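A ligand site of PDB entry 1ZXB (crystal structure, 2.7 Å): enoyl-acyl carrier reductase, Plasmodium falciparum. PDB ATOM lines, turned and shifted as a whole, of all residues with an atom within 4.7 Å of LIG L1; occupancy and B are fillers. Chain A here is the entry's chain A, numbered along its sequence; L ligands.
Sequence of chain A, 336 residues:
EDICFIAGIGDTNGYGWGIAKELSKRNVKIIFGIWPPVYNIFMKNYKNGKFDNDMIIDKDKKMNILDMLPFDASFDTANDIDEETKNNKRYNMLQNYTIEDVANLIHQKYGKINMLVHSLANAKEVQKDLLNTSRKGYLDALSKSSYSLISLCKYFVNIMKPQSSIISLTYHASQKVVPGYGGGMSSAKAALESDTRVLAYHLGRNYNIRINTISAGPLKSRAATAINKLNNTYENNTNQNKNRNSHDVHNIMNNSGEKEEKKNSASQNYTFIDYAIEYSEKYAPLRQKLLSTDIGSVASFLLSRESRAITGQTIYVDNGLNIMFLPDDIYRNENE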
ATOM      1  N   GLY A   8     -20.074 -19.508  15.026  1.00  0.00           N
ATOM      2  CA  GLY A   8     -21.243 -20.379  15.141  1.00  0.00           C
ATOM      3  C   GLY A   8     -22.592 -19.750  14.815  1.00  0.00           C
ATOM      4  O   GLY A   8     -23.543 -19.857  15.603  1.00  0.00           O
ATOM      5  N   ILE A   9     -22.665 -19.078  13.664  1.00  0.00           N
ATOM      6  CA  ILE A   9     -23.960 -18.765  13.079  1.00  0.00           C
ATOM      7  C   ILE A   9     -24.058 -19.256  11.630  1.00  0.00           C
ATOM      8  O   ILE A   9     -23.046 -19.565  10.976  1.00  0.00           O
ATOM      9  CB  ILE A   9     -24.375 -17.266  13.147  1.00  0.00           C
ATOM     10  CG1 ILE A   9     -23.699 -16.450  12.055  1.00  0.00           C
ATOM     11  CG2 ILE A   9     -24.160 -16.679  14.535  1.00  0.00           C
ATOM     12  CD1 ILE A   9     -24.446 -15.193  11.717  1.00  0.00           C
ATOM     13  N   GLY A  10     -25.319 -19.333  11.198  1.00  0.00           N
ATOM     14  CA  GLY A  10     -25.711 -19.675   9.838  1.00  0.00           C
ATOM     15  C   GLY A  10     -26.935 -18.854   9.437  1.00  0.00           C
ATOM     16  O   GLY A  10     -27.371 -18.895   8.288  1.00  0.00           O
ATOM     17  N   ASP A  11     -27.476 -18.077  10.389  1.00  0.00           N
ATOM     18  CA  ASP A  11     -28.668 -17.274  10.138  1.00  0.00           C
ATOM     19  C   ASP A  11     -28.957 -16.305  11.287  1.00  0.00           C
ATOM     20  O   ASP A  11     -28.141 -16.139  12.210  1.00  0.00           O
ATOM     21  CB  ASP A  11     -29.872 -18.185   9.934  1.00  0.00           C
ATOM     22  CG  ASP A  11     -29.996 -19.221  11.032  1.00  0.00           C
ATOM     23  OD1 ASP A  11     -29.967 -18.838  12.217  1.00  0.00           O
ATOM     24  OD2 ASP A  11     -30.116 -20.420  10.696  1.00  0.00           O
ATOM     25  N   ASN A  13     -31.579 -16.629  13.199  1.00  0.00           N
ATOM     26  CA  ASN A  13     -32.594 -17.348  13.952  1.00  0.00           C
ATOM     27  C   ASN A  13     -32.056 -17.959  15.232  1.00  0.00           C
ATOM     28  O   ASN A  13     -32.797 -18.573  16.012  1.00  0.00           O
ATOM     29  CB  ASN A  13     -33.244 -18.386  13.025  1.00  0.00           C
ATOM     30  CG  ASN A  13     -33.768 -17.737  11.737  1.00  0.00           C
ATOM     31  OD1 ASN A  13     -34.746 -16.997  11.782  1.00  0.00           O
ATOM     32  ND2 ASN A  13     -33.085 -17.954  10.608  1.00  0.00           N
ATOM     33  N   GLY A  14     -30.758 -17.722  15.478  1.00  0.00           N
ATOM     34  CA  GLY A  14     -30.049 -18.350  16.560  1.00  0.00           C
ATOM     35  C   GLY A  14     -29.568 -17.393  17.626  1.00  0.00           C
ATOM     36  O   GLY A  14     -29.899 -16.201  17.608  1.00  0.00           O
ATOM     37  N   TYR A  15     -28.799 -17.930  18.555  1.00  0.00           N
ATOM     38  CA  TYR A  15     -28.287 -17.178  19.692  1.00  0.00           C
ATOM     39  C   TYR A  15     -27.111 -16.270  19.353  1.00  0.00           C
ATOM     40  O   TYR A  15     -26.953 -15.209  19.961  1.00  0.00           O
ATOM     41  CB  TYR A  15     -27.929 -18.104  20.870  1.00  0.00           C
ATOM     42  CG  TYR A  15     -29.091 -18.447  21.778  1.00  0.00           C
ATOM     43  CD1 TYR A  15     -29.793 -17.434  22.434  1.00  0.00           C
ATOM     44  CD2 TYR A  15     -29.472 -19.771  22.011  1.00  0.00           C
ATOM     45  CE1 TYR A  15     -30.867 -17.731  23.279  1.00  0.00           C
ATOM     46  CE2 TYR A  15     -30.552 -20.077  22.866  1.00  0.00           C
ATOM     47  CZ  TYR A  15     -31.234 -19.045  23.498  1.00  0.00           C
ATOM     48  OH  TYR A  15     -32.297 -19.297  24.329  1.00  0.00           O
ATOM     49  N   GLY A  16     -26.287 -16.695  18.399  1.00  0.00           N
ATOM     50  CA  GLY A  16     -25.143 -15.902  17.978  1.00  0.00           C
ATOM     51  C   GLY A  16     -25.639 -14.564  17.505  1.00  0.00           C
ATOM     52  O   GLY A  16     -25.033 -13.534  17.792  1.00  0.00           O
ATOM     53  N   ILE A  34     -18.699 -18.530  10.100  1.00  0.00           N
ATOM     54  CA  ILE A  34     -19.775 -19.346   9.546  1.00  0.00           C
ATOM     55  C   ILE A  34     -19.206 -20.681   9.101  1.00  0.00           C
ATOM     56  O   ILE A  34     -18.193 -20.729   8.384  1.00  0.00           O
ATOM     57  CB  ILE A  34     -20.429 -18.661   8.339  1.00  0.00           C
ATOM     58  CG1 ILE A  34     -20.731 -17.190   8.626  1.00  0.00           C
ATOM     59  CG2 ILE A  34     -21.666 -19.411   7.857  1.00  0.00           C
ATOM     60  CD1 ILE A  34     -21.285 -16.975   9.984  1.00  0.00           C
ATOM     61  N   TRP A  35     -19.870 -21.760   9.531  1.00  0.00           N
ATOM     62  CA  TRP A  35     -19.609 -23.130   9.072  1.00  0.00           C
ATOM     63  C   TRP A  35     -19.660 -23.199   7.547  1.00  0.00           C
ATOM     64  O   TRP A  35     -20.710 -22.988   6.938  1.00  0.00           O
ATOM     65  CB  TRP A  35     -20.672 -24.025   9.677  1.00  0.00           C
ATOM     66  CG  TRP A  35     -20.549 -25.476   9.399  1.00  0.00           C
ATOM     67  CD1 TRP A  35     -19.437 -26.241   9.545  1.00  0.00           C
ATOM     68  CD2 TRP A  35     -21.607 -26.361   9.002  1.00  0.00           C
ATOM     69  NE1 TRP A  35     -19.727 -27.545   9.233  1.00  0.00           N
ATOM     70  CE2 TRP A  35     -21.056 -27.647   8.905  1.00  0.00           C
ATOM     71  CE3 TRP A  35     -22.965 -26.176   8.712  1.00  0.00           C
ATOM     72  CZ2 TRP A  35     -21.803 -28.770   8.524  1.00  0.00           C
ATOM     73  CZ3 TRP A  35     -23.711 -27.285   8.333  1.00  0.00           C
ATOM     74  CH2 TRP A  35     -23.124 -28.565   8.242  1.00  0.00           C
ATOM     75  N   PHE A  71     -15.612 -20.558   8.640  1.00  0.00           N
ATOM     76  CA  PHE A  71     -15.004 -21.055   9.877  1.00  0.00           C
ATOM     77  C   PHE A  71     -15.513 -22.432  10.249  1.00  0.00           C
ATOM     78  O   PHE A  71     -16.705 -22.599  10.444  1.00  0.00           O
ATOM     79  CB  PHE A  71     -15.266 -20.081  11.038  1.00  0.00           C
ATOM     80  CG  PHE A  71     -14.831 -20.613  12.393  1.00  0.00           C
ATOM     81  CD1 PHE A  71     -13.549 -20.385  12.871  1.00  0.00           C
ATOM     82  CD2 PHE A  71     -15.730 -21.339  13.197  1.00  0.00           C
ATOM     83  CE1 PHE A  71     -13.152 -20.877  14.115  1.00  0.00           C
ATOM     84  CE2 PHE A  71     -15.336 -21.837  14.434  1.00  0.00           C
ATOM     85  CZ  PHE A  71     -14.051 -21.607  14.895  1.00  0.00           C
ATOM     86  N   ASP A  72     -14.623 -23.407  10.365  1.00  0.00           N
ATOM     87  CA  ASP A  72     -15.014 -24.778  10.749  1.00  0.00           C
ATOM     88  C   ASP A  72     -14.373 -25.271  12.050  1.00  0.00           C
ATOM     89  O   ASP A  72     -13.167 -25.478  12.126  1.00  0.00           O
ATOM     90  CB  ASP A  72     -14.729 -25.779   9.628  1.00  0.00           C
ATOM     91  CG  ASP A  72     -15.391 -27.133   9.858  1.00  0.00           C
ATOM     92  OD1 ASP A  72     -15.365 -27.619  11.016  1.00  0.00           O
ATOM     93  OD2 ASP A  72     -15.941 -27.714   8.898  1.00  0.00           O
ATOM     94  N   ALA A  73     -15.210 -25.490  13.043  1.00  0.00           N
ATOM     95  CA  ALA A  73     -14.789 -25.809  14.408  1.00  0.00           C
ATOM     96  C   ALA A  73     -14.255 -27.227  14.588  1.00  0.00           C
ATOM     97  O   ALA A  73     -14.046 -27.668  15.738  1.00  0.00           O
ATOM     98  CB  ALA A  73     -15.950 -25.564  15.355  1.00  0.00           C
ATOM     99  N   SER A  74     -14.060 -27.947  13.497  1.00  0.00           N
ATOM    100  CA  SER A  74     -13.598 -29.343  13.582  1.00  0.00           C
ATOM    101  C   SER A  74     -12.164 -29.537  13.113  1.00  0.00           C
ATOM    102  O   SER A  74     -11.545 -30.553  13.420  1.00  0.00           O
ATOM    103  CB  SER A  74     -14.560 -30.312  12.871  1.00  0.00           C
ATOM    104  OG  SER A  74     -14.582 -30.114  11.471  1.00  0.00           O
ATOM    105  N   SER A 119     -20.377 -20.174  19.925  1.00  0.00           N
ATOM    106  CA  SER A 119     -21.830 -20.334  19.806  1.00  0.00           C
ATOM    107  C   SER A 119     -22.235 -21.409  18.801  1.00  0.00           C
ATOM    108  O   SER A 119     -23.170 -21.253  18.010  1.00  0.00           O
ATOM    109  CB  SER A 119     -22.511 -19.010  19.412  1.00  0.00           C
ATOM    110  OG  SER A 119     -23.919 -19.204  19.288  1.00  0.00           O
ATOM    111  N   LEU A 120     -21.533 -22.525  18.855  1.00  0.00           N
ATOM    112  CA  LEU A 120     -21.758 -23.557  17.900  1.00  0.00           C
ATOM    113  C   LEU A 120     -21.884 -24.860  18.616  1.00  0.00           C
ATOM    114  O   LEU A 120     -21.327 -25.038  19.699  1.00  0.00           O
ATOM    115  CB  LEU A 120     -20.608 -23.614  16.900  1.00  0.00           C
ATOM    116  CG  LEU A 120     -19.201 -23.655  17.487  1.00  0.00           C
ATOM    117  CD1 LEU A 120     -18.717 -25.085  17.522  1.00  0.00           C
ATOM    118  CD2 LEU A 120     -18.290 -22.755  16.672  1.00  0.00           C
ATOM    119  N   ALA A 121     -22.632 -25.766  18.005  1.00  0.00           N
ATOM    120  CA  ALA A 121     -22.745 -27.131  18.493  1.00  0.00           C
ATOM    121  C   ALA A 121     -23.123 -28.060  17.345  1.00  0.00           C
ATOM    122  O   ALA A 121     -23.671 -27.627  16.324  1.00  0.00           O
ATOM    123  CB  ALA A 121     -23.768 -27.224  19.628  1.00  0.00           C
ATOM    124  N   ASN A 122     -22.777 -29.326  17.513  1.00  0.00           N
ATOM    125  CA  ASN A 122     -23.205 -30.377  16.621  1.00  0.00           C
ATOM    126  C   ASN A 122     -23.028 -31.740  17.281  1.00  0.00           C
ATOM    127  O   ASN A 122     -21.965 -32.049  17.786  1.00  0.00           O
ATOM    128  CB  ASN A 122     -22.445 -30.299  15.275  1.00  0.00           C
ATOM    129  CG  ASN A 122     -23.212 -30.939  14.145  1.00  0.00           C
ATOM    130  OD1 ASN A 122     -23.219 -32.156  14.005  1.00  0.00           O
ATOM    131  ND2 ASN A 122     -23.863 -30.110  13.323  1.00  0.00           N
ATOM    132  N   LYS A 144     -16.778 -31.500  17.874  1.00  0.00           N
ATOM    133  CA  LYS A 144     -17.502 -30.354  17.385  1.00  0.00           C
ATOM    134  C   LYS A 144     -17.970 -29.397  18.514  1.00  0.00           C
ATOM    135  O   LYS A 144     -17.804 -28.193  18.390  1.00  0.00           O
ATOM    136  CB  LYS A 144     -18.666 -30.842  16.496  1.00  0.00           C
ATOM    137  CG  LYS A 144     -18.365 -30.858  14.963  1.00  0.00           C
ATOM    138  CD  LYS A 144     -17.534 -32.071  14.482  1.00  0.00           C
ATOM    139  CE  LYS A 144     -17.455 -32.172  12.939  1.00  0.00           C
ATOM    140  NZ  LYS A 144     -18.771 -32.389  12.263  1.00  0.00           N
ATOM    141  N   LEU A 169     -22.065 -21.053  24.894  1.00  0.00           N
ATOM    142  CA  LEU A 169     -23.416 -21.417  25.317  1.00  0.00           C
ATOM    143  C   LEU A 169     -23.483 -22.848  25.772  1.00  0.00           C
ATOM    144  O   LEU A 169     -22.672 -23.675  25.340  1.00  0.00           O
ATOM    145  CB  LEU A 169     -24.453 -21.219  24.224  1.00  0.00           C
ATOM    146  CG  LEU A 169     -24.826 -19.807  23.828  1.00  0.00           C
ATOM    147  CD1 LEU A 169     -24.702 -18.846  24.993  1.00  0.00           C
ATOM    148  CD2 LEU A 169     -23.939 -19.358  22.710  1.00  0.00           C
ATOM    149  N   THR A 170     -24.451 -23.160  26.624  1.00  0.00           N
ATOM    150  CA  THR A 170     -24.622 -24.511  27.154  1.00  0.00           C
ATOM    151  C   THR A 170     -26.063 -24.774  27.617  1.00  0.00           C
ATOM    152  O   THR A 170     -26.884 -23.845  27.739  1.00  0.00           O
ATOM    153  CB  THR A 170     -23.610 -24.831  28.289  1.00  0.00           C
ATOM    154  OG1 THR A 170     -23.778 -26.182  28.736  1.00  0.00           O
ATOM    155  CG2 THR A 170     -23.811 -23.882  29.430  1.00  0.00           C
ATOM    156  N   TYR A 171     -26.367 -26.035  27.860  1.00  0.00           N
ATOM    157  CA  TYR A 171     -27.703 -26.409  28.176  1.00  0.00           C
ATOM    158  C   TYR A 171     -27.749 -27.334  29.380  1.00  0.00           C
ATOM    159  O   TYR A 171     -26.965 -28.281  29.492  1.00  0.00           O
ATOM    160  CB  TYR A 171     -28.390 -26.979  26.927  1.00  0.00           C
ATOM    161  CG  TYR A 171     -29.850 -27.280  27.102  1.00  0.00           C
ATOM    162  CD1 TYR A 171     -30.745 -26.292  27.508  1.00  0.00           C
ATOM    163  CD2 TYR A 171     -30.345 -28.564  26.877  1.00  0.00           C
ATOM    164  CE1 TYR A 171     -32.094 -26.571  27.686  1.00  0.00           C
ATOM    165  CE2 TYR A 171     -31.697 -28.850  27.047  1.00  0.00           C
ATOM    166  CZ  TYR A 171     -32.556 -27.855  27.459  1.00  0.00           C
ATOM    167  OH  TYR A 171     -33.889 -28.136  27.645  1.00  0.00           O
ATOM    168  N   TYR A 181     -32.405 -35.348  24.248  1.00  0.00           N
ATOM    169  CA  TYR A 181     -31.185 -34.594  24.013  1.00  0.00           C
ATOM    170  C   TYR A 181     -29.987 -35.540  23.876  1.00  0.00           C
ATOM    171  O   TYR A 181     -29.022 -35.478  24.654  1.00  0.00           O
ATOM    172  CB  TYR A 181     -30.958 -33.601  25.163  1.00  0.00           C
ATOM    173  CG  TYR A 181     -29.981 -32.483  24.890  1.00  0.00           C
ATOM    174  CD1 TYR A 181     -30.318 -31.429  24.062  1.00  0.00           C
ATOM    175  CD2 TYR A 181     -28.715 -32.484  25.452  1.00  0.00           C
ATOM    176  CE1 TYR A 181     -29.445 -30.401  23.813  1.00  0.00           C
ATOM    177  CE2 TYR A 181     -27.806 -31.450  25.209  1.00  0.00           C
ATOM    178  CZ  TYR A 181     -28.194 -30.412  24.389  1.00  0.00           C
ATOM    179  OH  TYR A 181     -27.327 -29.368  24.129  1.00  0.00           O
ATOM    180  N   MET A 185     -24.714 -34.895  23.046  1.00  0.00           N
ATOM    181  CA  MET A 185     -24.820 -33.459  23.289  1.00  0.00           C
ATOM    182  C   MET A 185     -24.707 -33.134  24.784  1.00  0.00           C
ATOM    183  O   MET A 185     -23.914 -32.280  25.186  1.00  0.00           O
ATOM    184  CB  MET A 185     -26.120 -32.887  22.741  1.00  0.00           C
ATOM    185  CG  MET A 185     -25.996 -32.031  21.478  1.00  0.00           C
ATOM    186  SD  MET A 185     -24.565 -30.940  21.341  1.00  0.00           S
ATOM    187  CE  MET A 185     -24.763 -30.001  22.842  1.00  0.00           C
ATOM    188  N   LYS A 189     -22.028 -30.982  26.531  1.00  0.00           N
ATOM    189  CA  LYS A 189     -22.280 -29.793  27.350  1.00  0.00           C
ATOM    190  C   LYS A 189     -21.614 -29.904  28.725  1.00  0.00           C
ATOM    191  O   LYS A 189     -21.066 -28.927  29.244  1.00  0.00           O
ATOM    192  CB  LYS A 189     -23.787 -29.512  27.469  1.00  0.00           C
ATOM    193  CG  LYS A 189     -24.437 -29.006  26.174  1.00  0.00           C
ATOM    194  CD  LYS A 189     -23.632 -27.883  25.565  1.00  0.00           C
ATOM    195  CE  LYS A 189     -24.439 -27.082  24.522  1.00  0.00           C
ATOM    196  NZ  LYS A 189     -23.606 -26.078  23.725  1.00  0.00           N
ATOM    197  N   ALA A 216     -28.461 -21.346  28.444  1.00  0.00           N
ATOM    198  CA  ALA A 216     -29.709 -20.752  27.978  1.00  0.00           C
ATOM    199  C   ALA A 216     -30.912 -21.696  28.059  1.00  0.00           C
ATOM    200  O   ALA A 216     -30.770 -22.886  28.281  1.00  0.00           O
ATOM    201  CB  ALA A 216     -29.553 -20.253  26.582  1.00  0.00           C
ATOM    202  N   GLY A 217     -32.095 -21.108  27.896  1.00  0.00           N
ATOM    203  CA  GLY A 217     -33.341 -21.843  27.840  1.00  0.00           C
ATOM    204  C   GLY A 217     -33.653 -22.098  26.389  1.00  0.00           C
ATOM    205  O   GLY A 217     -32.910 -21.669  25.513  1.00  0.00           O
ATOM    206  N   PRO A 218     -34.753 -22.810  26.115  1.00  0.00           N
ATOM    207  CA  PRO A 218     -34.999 -23.253  24.759  1.00  0.00           C
ATOM    208  C   PRO A 218     -35.297 -22.053  23.878  1.00  0.00           C
ATOM    209  O   PRO A 218     -35.873 -21.061  24.359  1.00  0.00           O
ATOM    210  CB  PRO A 218     -36.240 -24.147  24.885  1.00  0.00           C
ATOM    211  CG  PRO A 218     -36.933 -23.687  26.147  1.00  0.00           C
ATOM    212  CD  PRO A 218     -35.825 -23.237  27.051  1.00  0.00           C
ATOM    213  N   LEU A 219     -34.867 -22.137  22.630  1.00  0.00           N
ATOM    214  CA  LEU A 219     -35.104 -21.106  21.640  1.00  0.00           C
ATOM    215  C   LEU A 219     -35.248 -21.778  20.290  1.00  0.00           C
ATOM    216  O   LEU A 219     -34.356 -22.512  19.856  1.00  0.00           O
ATOM    217  CB  LEU A 219     -33.952 -20.105  21.603  1.00  0.00           C
ATOM    218  CG  LEU A 219     -33.941 -19.069  20.460  1.00  0.00           C
ATOM    219  CD1 LEU A 219     -34.838 -17.828  20.731  1.00  0.00           C
ATOM    220  CD2 LEU A 219     -32.515 -18.655  20.127  1.00  0.00           C
ATOM    221  N   SER A 221     -34.434 -21.958  17.349  1.00  0.00           N
ATOM    222  CA  SER A 221     -33.424 -21.656  16.336  1.00  0.00           C
ATOM    223  C   SER A 221     -33.457 -22.746  15.263  1.00  0.00           C
ATOM    224  O   SER A 221     -34.118 -23.782  15.440  1.00  0.00           O
ATOM    225  CB  SER A 221     -32.058 -21.607  16.991  1.00  0.00           C
ATOM    226  OG  SER A 221     -31.697 -22.863  17.523  1.00  0.00           O
ATOM    227  N   ARG A 222     -32.741 -22.531  14.164  1.00  0.00           N
ATOM    228  CA  ARG A 222     -32.676 -23.511  13.081  1.00  0.00           C
ATOM    229  C   ARG A 222     -32.256 -24.892  13.595  1.00  0.00           C
ATOM    230  O   ARG A 222     -32.919 -25.895  13.311  1.00  0.00           O
ATOM    231  CB  ARG A 222     -31.750 -23.053  11.953  1.00  0.00           C
ATOM    232  CG  ARG A 222     -32.352 -23.171  10.531  1.00  0.00           C
ATOM    233  CD  ARG A 222     -31.398 -23.893   9.557  1.00  0.00           C
ATOM    234  NE  ARG A 222     -31.483 -25.362   9.683  1.00  0.00           N
ATOM    235  CZ  ARG A 222     -30.619 -26.148  10.335  1.00  0.00           C
ATOM    236  NH1 ARG A 222     -29.541 -25.632  10.928  1.00  0.00           N
ATOM    237  NH2 ARG A 222     -30.826 -27.454  10.383  1.00  0.00           N
ATOM    238  N   ALA A 223     -31.178 -24.945  14.376  1.00  0.00           N
ATOM    239  CA  ALA A 223     -30.661 -26.202  14.924  1.00  0.00           C
ATOM    240  C   ALA A 223     -31.557 -26.850  15.990  1.00  0.00           C
ATOM    241  O   ALA A 223     -31.594 -28.084  16.121  1.00  0.00           O
ATOM    242  CB  ALA A 223     -29.263 -25.997  15.450  1.00  0.00           C
ATOM    243  N   ALA A 224     -32.260 -26.037  16.766  1.00  0.00           N
ATOM    244  CA  ALA A 224     -33.217 -26.558  17.756  1.00  0.00           C
ATOM    245  C   ALA A 224     -34.352 -27.356  17.090  1.00  0.00           C
ATOM    246  O   ALA A 224     -34.826 -28.370  17.616  1.00  0.00           O
ATOM    247  CB  ALA A 224     -33.782 -25.424  18.593  1.00  0.00           C
ATOM    248  N   ILE A 273     -38.312 -29.272  20.645  1.00  0.00           N
ATOM    249  CA  ILE A 273     -38.121 -27.871  20.936  1.00  0.00           C
ATOM    250  C   ILE A 273     -39.437 -27.161  21.154  1.00  0.00           C
ATOM    251  O   ILE A 273     -39.476 -26.163  21.870  1.00  0.00           O
ATOM    252  CB  ILE A 273     -37.225 -27.168  19.879  1.00  0.00           C
ATOM    253  CG1 ILE A 273     -36.803 -25.779  20.378  1.00  0.00           C
ATOM    254  CG2 ILE A 273     -37.908 -27.080  18.557  1.00  0.00           C
ATOM    255  CD1 ILE A 273     -35.840 -25.805  21.555  1.00  0.00           C
HETATM  256  P1  LIG L   1     -27.952 -22.107  15.505  1.00  0.00           P
HETATM  257  O1  LIG L   1     -28.328 -23.005  14.345  1.00  0.00           O
HETATM  258  O2  LIG L   1     -28.293 -20.640  15.513  1.00  0.00           O
HETATM  259  O3  LIG L   1     -26.361 -22.073  15.693  1.00  0.00           O
HETATM  260  C1  LIG L   1     -25.651 -23.279  15.857  1.00  0.00           C
HETATM  261  C2  LIG L   1     -24.551 -23.157  14.856  1.00  0.00           C
HETATM  262  O4  LIG L   1     -23.511 -24.089  15.142  1.00  0.00           O
HETATM  263  C3  LIG L   1     -25.054 -23.469  13.439  1.00  0.00           C
HETATM  264  O5  LIG L   1     -24.970 -22.299  12.618  1.00  0.00           O
HETATM  265  C4  LIG L   1     -24.092 -24.516  12.956  1.00  0.00           C
HETATM  266  O6  LIG L   1     -23.684 -24.311  11.606  1.00  0.00           O
HETATM  267  C5  LIG L   1     -22.919 -24.208  13.852  1.00  0.00           C
HETATM  268  N1  LIG L   1     -21.829 -25.170  13.679  1.00  0.00           N
HETATM  269  C6  LIG L   1     -21.876 -26.522  13.789  1.00  0.00           C
HETATM  270  N2  LIG L   1     -20.655 -27.060  13.528  1.00  0.00           N
HETATM  271  C7  LIG L   1     -19.817 -26.039  13.231  1.00  0.00           C
HETATM  272  C8  LIG L   1     -18.485 -25.938  12.880  1.00  0.00           C
HETATM  273  N3  LIG L   1     -17.742 -27.066  12.789  1.00  0.00           N
HETATM  274  N4  LIG L   1     -17.952 -24.706  12.641  1.00  0.00           N
HETATM  275  C9  LIG L   1     -18.685 -23.563  12.729  1.00  0.00           C
HETATM  276  N5  LIG L   1     -19.997 -23.589  13.066  1.00  0.00           N
HETATM  277  C10 LIG L   1     -20.594 -24.789  13.319  1.00  0.00           C
HETATM  278  O7  LIG L   1     -28.529 -22.821  16.853  1.00  0.00           O
HETATM  279  P2  LIG L   1     -28.423 -22.243  18.377  1.00  0.00           P
HETATM  280  O8  LIG L   1     -28.594 -20.755  18.347  1.00  0.00           O
HETATM  281  O9  LIG L   1     -29.309 -23.082  19.253  1.00  0.00           O
HETATM  282  O10 LIG L   1     -26.908 -22.612  18.788  1.00  0.00           O
HETATM  283  C11 LIG L   1     -26.109 -21.695  19.544  1.00  0.00           C
HETATM  284  C12 LIG L   1     -25.642 -22.386  20.824  1.00  0.00           C
HETATM  285  O11 LIG L   1     -26.657 -22.335  21.824  1.00  0.00           O
HETATM  286  C13 LIG L   1     -25.357 -23.852  20.595  1.00  0.00           C
HETATM  287  O12 LIG L   1     -24.116 -24.184  21.205  1.00  0.00           O
HETATM  288  C14 LIG L   1     -26.479 -24.572  21.316  1.00  0.00           C
HETATM  289  O13 LIG L   1     -26.019 -25.850  21.728  1.00  0.00           O
HETATM  290  C15 LIG L   1     -26.795 -23.624  22.452  1.00  0.00           C
HETATM  291  N6  LIG L   1     -28.128 -23.722  23.046  1.00  0.00           N
HETATM  292  C16 LIG L   1     -29.248 -23.499  22.323  1.00  0.00           C
HETATM  293  C17 LIG L   1     -30.515 -23.558  22.898  1.00  0.00           C
HETATM  294  C18 LIG L   1     -31.742 -23.342  22.076  1.00  0.00           C
HETATM  295  O14 LIG L   1     -32.927 -23.815  22.475  1.00  0.00           O
HETATM  296  N7  LIG L   1     -31.680 -22.715  20.984  1.00  0.00           N
HETATM  297  C19 LIG L   1     -30.629 -23.836  24.260  1.00  0.00           C
HETATM  298  C20 LIG L   1     -29.472 -24.052  24.989  1.00  0.00           C
HETATM  299  C21 LIG L   1     -28.235 -23.977  24.360  1.00  0.00           C
HETATM  300 CL1  LG2 L   2     -26.513 -25.890  18.035  1.00  0.00          CL
HETATM  301  C1  LG2 L   2     -27.384 -27.444  18.084  1.00  0.00           C
HETATM  302  C2  LG2 L   2     -27.216 -28.397  17.098  1.00  0.00           C
HETATM  303  C3  LG2 L   2     -27.904 -29.613  17.146  1.00  0.00           C
HETATM  304  C4  LG2 L   2     -27.650 -30.567  16.041  1.00  0.00           C
HETATM  305  O1  LG2 L   2     -26.863 -30.242  15.190  1.00  0.00           O
HETATM  306  N1  LG2 L   2     -28.227 -31.747  15.917  1.00  0.00           N
HETATM  307  C5  LG2 L   2     -27.913 -32.629  14.809  1.00  0.00           C
HETATM  308  C6  LG2 L   2     -28.778 -29.877  18.191  1.00  0.00           C
HETATM  309  C7  LG2 L   2     -28.937 -28.909  19.175  1.00  0.00           C
HETATM  310  C8  LG2 L   2     -28.249 -27.693  19.127  1.00  0.00           C
HETATM  311  O2  LG2 L   2     -28.386 -26.704  20.071  1.00  0.00           O
HETATM  312  C9  LG2 L   2     -29.424 -26.740  20.988  1.00  0.00           C
HETATM  313  C10 LG2 L   2     -29.147 -27.039  22.319  1.00  0.00           C
HETATM  314  O3  LG2 L   2     -27.865 -27.292  22.711  1.00  0.00           O
HETATM  315  C11 LG2 L   2     -30.166 -27.085  23.250  1.00  0.00           C
HETATM  316  C12 LG2 L   2     -30.750 -26.495  20.595  1.00  0.00           C
HETATM  317  C13 LG2 L   2     -31.778 -26.555  21.528  1.00  0.00           C
HETATM  318  C14 LG2 L   2     -31.480 -26.847  22.856  1.00  0.00           C
HETATM  319 CL2  LG2 L   2     -32.761 -26.967  24.098  1.00  0.00          CL
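A nitrogen (N4) of LIG L1 lies close to the backbone carbonyl oxygen of Phe 71 (3.3 Å). Residues that only touch LIG L1: Gly 14, Pro 218, Ser 119, Ile 9, Gly 217, Leu 169, Trp 35, Gly 8, Tyr 171, Thr 170, Ile 273, Ala 216 and Ser 74. Within 4 Å of LIG L1: Gly 8, Ile 9, Gly 10, Gly 14, Tyr 15, Trp 35, Phe 71, Asp 72, Ala 73, Ser 74, Ser 119, Leu 120, Ala 121, Leu 169, Thr 170, Tyr 171, Lys 189, Ala 216, Gly 217, Pro 218, Leu 219, Ser 221, Ala 223 and Ile 273.
The side-chain hydroxyl (OH) of Tyr 15 lies within hydrogen-bond range of the backbone carbonyl oxygen (O) of Gly 217. The backbone NH (N) of Ala 224 sits at hydrogen-bond distance from the side-chain hydroxyl (OG) of Ser 221, 3.3 Å away. OD1 of Asp 72 is in hydrogen-bond range of OG of Ser 74. NZ of Lys 189 sits at hydrogen-bond distance from O of Leu 169 (3.0 Å). The backbone carbonyl oxygen (O) of Phe 71 lies close to the backbone NH (N) of Trp 35, 3.4 Å away. The backbone carbonyl oxygen of Ile 34 lies within hydrogen-bond range of the backbone NH of Phe 71, 2.6 Å away. The backbone NH (N) of Ala 216 sits at hydrogen-bond distance from the backbone carbonyl oxygen (O) of Thr 170 (3.0 Å).
An oxygen (O14) of LIG L1 lies within hydrogen-bond range of the backbone NH of Leu 219, 2.6 Å away. O of Leu 219 is in hydrogen-bond range of N7 of LIG L1. N of Tyr 15 lies within hydrogen-bond range of O8 of LIG L1. A nitrogen (N4) of LIG L1 is in hydrogen-bond range of the backbone NH of Ala 73 (2.9 Å). OG of Ser 221 lies within hydrogen-bond range of O9 of LIG L1 (3.0 Å). The side-chain carboxylate (OD1) of Asp 72 lies within hydrogen-bond range of a nitrogen (N3) of LIG L1 (3.0 Å). The side-chain amino group of Lys 189 sits at hydrogen-bond distance from an oxygen (O13) of LIG L1. The backbone carbonyl oxygen (O) of Leu 120 lies within hydrogen-bond range of an oxygen (O12) of LIG L1 (3.3 Å). The backbone NH (N) of Ala 121 is in hydrogen-bond range of an oxygen (O4) of LIG L1. The backbone NH of Gly 10 is in hydrogen-bond range of an oxygen (O5) of LIG L1 (3.3 Å). An oxygen (O1) of LIG L1 lies close to the backbone NH (N) of Ala 223. O3 of LG2 L2 sits at hydrogen-bond distance from OH of Tyr 181 (2.6 Å).
An oxygen (O13) of LIG L1 sits at hydrogen-bond distance from an oxygen (O3) of LG2 L2 (2.5 Å).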
